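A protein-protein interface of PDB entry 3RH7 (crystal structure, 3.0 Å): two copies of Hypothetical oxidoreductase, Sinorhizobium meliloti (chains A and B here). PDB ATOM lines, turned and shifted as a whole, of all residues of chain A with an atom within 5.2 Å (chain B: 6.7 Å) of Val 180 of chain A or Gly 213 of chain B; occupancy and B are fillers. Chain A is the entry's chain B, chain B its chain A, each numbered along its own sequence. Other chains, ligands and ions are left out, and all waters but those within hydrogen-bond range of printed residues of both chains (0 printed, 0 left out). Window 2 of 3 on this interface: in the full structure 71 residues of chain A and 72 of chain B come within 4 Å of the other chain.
The side-chain hydroxyl of Thr 219 of chain B lies within hydrogen-bond range of the backbone carbonyl oxygen of Asp 215 of chain B (3.0 Å).
Among the printed residues, pairs that only touch across the chains: Ser 177 of chain A with Gly 214 of chain B (3.3 Å), Ala 179 of chain A with Val 176 of chain B (3.4 Å), Val 180 of chain A with Ala 179 of chain B (3.5 Å), Val 176 of chain A with Ala 179 of chain B (3.5 Å), Ser 177 of chain A with Asp 215 of chain B (3.5 Å), Ala 179 of chain A with Val 180 of chain B (3.5 Å), Val 180 of chain A with Gly 213 of chain B (3.5 Å), Val 176 of chain A with Pro 216 of chain B (3.6 Å), Ala 175 of chain A with Val 176 of chain B (3.8 Å) and Val 176 of chain A with Val 176 of chain B (3.9 Å).
Of the printed residues of chain B, Ala 179 of chain A touches Val 176 (3.4 Å) and Val 180 (3.5 Å).
Of chain A, only Val 180 (3.5 Å) comes within 4 Å of Gly 213 of chain B.
Of the printed residues of chain A, Gly 214 of chain B touches Ser 177.
The nearest residue of chain B that does not touch Val 180 of chain A is Glu 212 of chain B (4.3 Å).
The nearest printed residue of chain A that does not touch Gly 213 of chain B is Ser 177 of chain A (5.3 Å).
Printed residues of chain B that touch a printed residue of chain A: Val 176, Ala 179, Val 180, Gly 213, Gly 214, Asp 215 and Pro 216.
Hydrophobic or aromatic side chains of chain B within 4 Å of the printed part of chain A: Val 176, Ala 179, Val 180 and Pro 216.
Of the 8 printed residues of chain A, 5 touch a printed residue of chain B.
Hydrophobic or aromatic side chains of chain A that line the printed part of chain B: Ala 175, Val 176, Ala 179 and Val 180.
Along chain A the printed residues that touch a printed residue of chain B span positions 175 to 180.
Among the printed residues, 10 pairs touch across the chains.
Val 176 of chain A touches its own counterpart, Val 176 of chain B.
Val 176 of chain A touches Ala 179 of chain B, and with the chains exchanged Ala 179 of chain A touches Val 176 of chain B.
Ala 179 of chain A touches Val 180 of chain B, and with the chains exchanged Val 180 of chain A touches Ala 179 of chain B.
Of the 10 pairs that touch across the chains among the printed residues, 5 have their exchanged pair printed and touching as well.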
ATOM      1  N   ALA A 175       1.878 -26.512  -1.517  1.00  0.00           N
ATOM      2  CA  ALA A 175       2.895 -27.352  -0.899  1.00  0.00           C
ATOM      3  C   ALA A 175       3.627 -26.606   0.175  1.00  0.00           C
ATOM      4  O   ALA A 175       3.742 -27.106   1.282  1.00  0.00           O
ATOM      5  CB  ALA A 175       3.882 -27.827  -1.958  1.00  0.00           C
ATOM      6  N   VAL A 176       4.107 -25.397  -0.141  1.00  0.00           N
ATOM      7  CA  VAL A 176       4.840 -24.518   0.776  1.00  0.00           C
ATOM      8  C   VAL A 176       3.961 -24.207   2.001  1.00  0.00           C
ATOM      9  O   VAL A 176       4.440 -24.373   3.111  1.00  0.00           O
ATOM     10  CB  VAL A 176       5.319 -23.233   0.046  1.00  0.00           C
ATOM     11  CG1 VAL A 176       5.878 -22.208   1.008  1.00  0.00           C
ATOM     12  CG2 VAL A 176       6.348 -23.572  -1.021  1.00  0.00           C
ATOM     13  N   SER A 177       2.674 -23.853   1.811  1.00  0.00           N
ATOM     14  CA  SER A 177       1.783 -23.557   2.933  1.00  0.00           C
ATOM     15  C   SER A 177       1.703 -24.720   3.892  1.00  0.00           C
ATOM     16  O   SER A 177       1.878 -24.523   5.096  1.00  0.00           O
ATOM     17  CB  SER A 177       0.386 -23.190   2.459  1.00  0.00           C
ATOM     18  OG  SER A 177      -0.377 -22.760   3.578  1.00  0.00           O
ATOM     19  N   ALA A 178       1.515 -25.934   3.343  1.00  0.00           N
ATOM     20  CA  ALA A 178       1.415 -27.223   4.047  1.00  0.00           C
ATOM     21  C   ALA A 178       2.673 -27.541   4.815  1.00  0.00           C
ATOM     22  O   ALA A 178       2.598 -27.920   5.983  1.00  0.00           O
ATOM     23  CB  ALA A 178       1.122 -28.346   3.052  1.00  0.00           C
ATOM     24  N   ALA A 179       3.823 -27.389   4.160  1.00  0.00           N
ATOM     25  CA  ALA A 179       5.152 -27.671   4.716  1.00  0.00           C
ATOM     26  C   ALA A 179       5.445 -26.894   6.011  1.00  0.00           C
ATOM     27  O   ALA A 179       6.054 -27.433   6.938  1.00  0.00           O
ATOM     28  CB  ALA A 179       6.209 -27.335   3.684  1.00  0.00           C
ATOM     29  N   VAL A 180       4.990 -25.643   6.073  1.00  0.00           N
ATOM     30  CA  VAL A 180       5.196 -24.752   7.212  1.00  0.00           C
ATOM     31  C   VAL A 180       4.228 -25.123   8.356  1.00  0.00           C
ATOM     32  O   VAL A 180       4.622 -24.985   9.521  1.00  0.00           O
ATOM     33  CB  VAL A 180       5.086 -23.267   6.781  1.00  0.00           C
ATOM     34  CG1 VAL A 180       5.164 -22.336   7.968  1.00  0.00           C
ATOM     35  CG2 VAL A 180       6.166 -22.907   5.766  1.00  0.00           C
ATOM     36  N   GLU A 181       3.007 -25.647   8.029  1.00  0.00           N
ATOM     37  CA  GLU A 181       1.970 -26.055   8.992  1.00  0.00           C
ATOM     38  C   GLU A 181       2.475 -27.157   9.957  1.00  0.00           C
ATOM     39  O   GLU A 181       2.076 -27.185  11.123  1.00  0.00           O
ATOM     40  CB  GLU A 181       0.701 -26.530   8.246  1.00  0.00           C
ATOM     41  CG  GLU A 181      -0.476 -25.568   8.305  1.00  0.00           C
ATOM     42  CD  GLU A 181      -1.672 -25.971   7.464  1.00  0.00           C
ATOM     43  OE1 GLU A 181      -2.408 -26.892   7.890  1.00  0.00           O
ATOM     44  OE2 GLU A 181      -1.869 -25.376   6.377  1.00  0.00           O
ATOM     45  N   GLY A 182       3.341 -28.037   9.459  1.00  0.00           N
ATOM     46  CA  GLY A 182       3.918 -29.124  10.234  1.00  0.00           C
ATOM     47  C   GLY A 182       4.449 -30.204   9.329  1.00  0.00           C
ATOM     48  O   GLY A 182       4.802 -29.929   8.176  1.00  0.00           O
ATOM     49  N   VAL B 176       9.838 -25.341  -0.794  1.00  0.00           N
ATOM     50  CA  VAL B 176       9.363 -26.067   0.382  1.00  0.00           C
ATOM     51  C   VAL B 176      10.518 -26.197   1.421  1.00  0.00           C
ATOM     52  O   VAL B 176      10.316 -25.892   2.597  1.00  0.00           O
ATOM     53  CB  VAL B 176       8.751 -27.445  -0.017  1.00  0.00           C
ATOM     54  CG1 VAL B 176       8.393 -28.259   1.211  1.00  0.00           C
ATOM     55  CG2 VAL B 176       7.514 -27.281  -0.896  1.00  0.00           C
ATOM     56  N   ALA B 178      13.147 -24.267   1.848  1.00  0.00           N
ATOM     57  CA  ALA B 178      13.384 -22.898   2.306  1.00  0.00           C
ATOM     58  C   ALA B 178      12.320 -22.433   3.287  1.00  0.00           C
ATOM     59  O   ALA B 178      12.643 -21.846   4.324  1.00  0.00           O
ATOM     60  CB  ALA B 178      13.423 -21.955   1.120  1.00  0.00           C
ATOM     61  N   ALA B 179      11.051 -22.689   2.956  1.00  0.00           N
ATOM     62  CA  ALA B 179       9.885 -22.303   3.750  1.00  0.00           C
ATOM     63  C   ALA B 179       9.932 -22.864   5.172  1.00  0.00           C
ATOM     64  O   ALA B 179       9.528 -22.179   6.115  1.00  0.00           O
ATOM     65  CB  ALA B 179       8.627 -22.785   3.054  1.00  0.00           C
ATOM     66  N   VAL B 180      10.446 -24.089   5.317  1.00  0.00           N
ATOM     67  CA  VAL B 180      10.519 -24.754   6.611  1.00  0.00           C
ATOM     68  C   VAL B 180      11.702 -24.200   7.437  1.00  0.00           C
ATOM     69  O   VAL B 180      11.599 -24.143   8.670  1.00  0.00           O
ATOM     70  CB  VAL B 180      10.572 -26.295   6.461  1.00  0.00           C
ATOM     71  CG1 VAL B 180      10.761 -26.981   7.820  1.00  0.00           C
ATOM     72  CG2 VAL B 180       9.317 -26.820   5.739  1.00  0.00           C
ATOM     73  N   GLY B 182      12.703 -21.179   7.816  1.00  0.00           N
ATOM     74  CA  GLY B 182      12.299 -19.980   8.529  1.00  0.00           C
ATOM     75  C   GLY B 182      11.520 -19.045   7.646  1.00  0.00           C
ATOM     76  O   GLY B 182      10.921 -19.489   6.653  1.00  0.00           O
ATOM     77  N   GLU B 183      11.528 -17.741   7.998  1.00  0.00           N
ATOM     78  CA  GLU B 183      10.824 -16.712   7.220  1.00  0.00           C
ATOM     79  C   GLU B 183      11.394 -16.631   5.800  1.00  0.00           C
ATOM     80  O   GLU B 183      12.593 -16.880   5.598  1.00  0.00           O
ATOM     81  CB  GLU B 183      10.830 -15.324   7.902  1.00  0.00           C
ATOM     82  CG  GLU B 183      12.203 -14.692   7.975  1.00  0.00           C
ATOM     83  CD  GLU B 183      12.372 -13.317   8.598  1.00  0.00           C
ATOM     84  OE1 GLU B 183      11.424 -12.807   9.238  1.00  0.00           O
ATOM     85  OE2 GLU B 183      13.498 -12.780   8.492  1.00  0.00           O
ATOM     86  N   ILE B 184      10.523 -16.355   4.828  1.00  0.00           N
ATOM     87  CA  ILE B 184      10.916 -16.218   3.435  1.00  0.00           C
ATOM     88  C   ILE B 184      10.548 -14.812   2.930  1.00  0.00           C
ATOM     89  O   ILE B 184       9.492 -14.256   3.283  1.00  0.00           O
ATOM     90  CB  ILE B 184      10.296 -17.311   2.513  1.00  0.00           C
ATOM     91  CG1 ILE B 184       8.772 -17.423   2.755  1.00  0.00           C
ATOM     92  CG2 ILE B 184      11.034 -18.641   2.611  1.00  0.00           C
ATOM     93  CD1 ILE B 184       8.004 -18.705   2.370  1.00  0.00           C
ATOM     94  N   VAL B 211       7.351 -13.130   5.143  1.00  0.00           N
ATOM     95  CA  VAL B 211       6.350 -13.826   5.955  1.00  0.00           C
ATOM     96  C   VAL B 211       6.859 -15.215   6.341  1.00  0.00           C
ATOM     97  O   VAL B 211       7.875 -15.670   5.796  1.00  0.00           O
ATOM     98  CB  VAL B 211       4.998 -13.931   5.193  1.00  0.00           C
ATOM     99  CG1 VAL B 211       4.422 -12.554   4.878  1.00  0.00           C
ATOM    100  CG2 VAL B 211       5.138 -14.761   3.907  1.00  0.00           C
ATOM    101  N   GLU B 212       6.146 -15.900   7.259  1.00  0.00           N
ATOM    102  CA  GLU B 212       6.457 -17.287   7.648  1.00  0.00           C
ATOM    103  C   GLU B 212       5.146 -18.019   7.815  1.00  0.00           C
ATOM    104  O   GLU B 212       4.492 -17.904   8.854  1.00  0.00           O
ATOM    105  CB  GLU B 212       7.312 -17.362   8.913  1.00  0.00           C
ATOM    106  CG  GLU B 212       7.802 -18.764   9.255  1.00  0.00           C
ATOM    107  CD  GLU B 212       8.799 -18.904  10.399  1.00  0.00           C
ATOM    108  OE1 GLU B 212       9.139 -17.898  11.071  1.00  0.00           O
ATOM    109  OE2 GLU B 212       9.243 -20.055  10.617  1.00  0.00           O
ATOM    110  N   GLY B 213       4.739 -18.722   6.769  1.00  0.00           N
ATOM    111  CA  GLY B 213       3.483 -19.452   6.792  1.00  0.00           C
ATOM    112  C   GLY B 213       2.464 -18.875   5.854  1.00  0.00           C
ATOM    113  O   GLY B 213       2.407 -17.644   5.675  1.00  0.00           O
ATOM    114  N   GLY B 214       1.680 -19.793   5.264  1.00  0.00           N
ATOM    115  CA  GLY B 214       0.619 -19.513   4.309  1.00  0.00           C
ATOM    116  C   GLY B 214       1.040 -19.819   2.892  1.00  0.00           C
ATOM    117  O   GLY B 214       2.193 -20.201   2.663  1.00  0.00           O
ATOM    118  N   ASP B 215       0.095 -19.676   1.930  1.00  0.00           N
ATOM    119  CA  ASP B 215       0.371 -19.927   0.524  1.00  0.00           C
ATOM    120  C   ASP B 215       1.168 -18.745   0.011  1.00  0.00           C
ATOM    121  O   ASP B 215       0.678 -17.622   0.060  1.00  0.00           O
ATOM    122  CB  ASP B 215      -0.910 -20.173  -0.282  1.00  0.00           C
ATOM    123  CG  ASP B 215      -0.686 -20.720  -1.695  1.00  0.00           C
ATOM    124  OD1 ASP B 215       0.234 -20.205  -2.398  1.00  0.00           O
ATOM    125  OD2 ASP B 215      -1.489 -21.604  -2.136  1.00  0.00           O
ATOM    126  N   PRO B 216       2.444 -18.954  -0.366  1.00  0.00           N
ATOM    127  CA  PRO B 216       3.270 -17.829  -0.819  1.00  0.00           C
ATOM    128  C   PRO B 216       2.626 -17.077  -2.000  1.00  0.00           C
ATOM    129  O   PRO B 216       2.680 -15.827  -2.036  1.00  0.00           O
ATOM    130  CB  PRO B 216       4.604 -18.491  -1.200  1.00  0.00           C
ATOM    131  CG  PRO B 216       4.262 -19.923  -1.444  1.00  0.00           C
ATOM    132  CD  PRO B 216       3.193 -20.222  -0.445  1.00  0.00           C
ATOM    133  N   THR B 219      -0.411 -14.978  -0.575  1.00  0.00           N
ATOM    134  CA  THR B 219       0.190 -13.883   0.191  1.00  0.00           C
ATOM    135  C   THR B 219       0.709 -12.768  -0.753  1.00  0.00           C
ATOM    136  O   THR B 219       0.392 -11.574  -0.575  1.00  0.00           O
ATOM    137  CB  THR B 219       1.309 -14.440   1.069  1.00  0.00           C
ATOM    138  OG1 THR B 219       0.762 -15.385   1.982  1.00  0.00           O
ATOM    139  CG2 THR B 219       2.054 -13.356   1.840  1.00  0.00           C
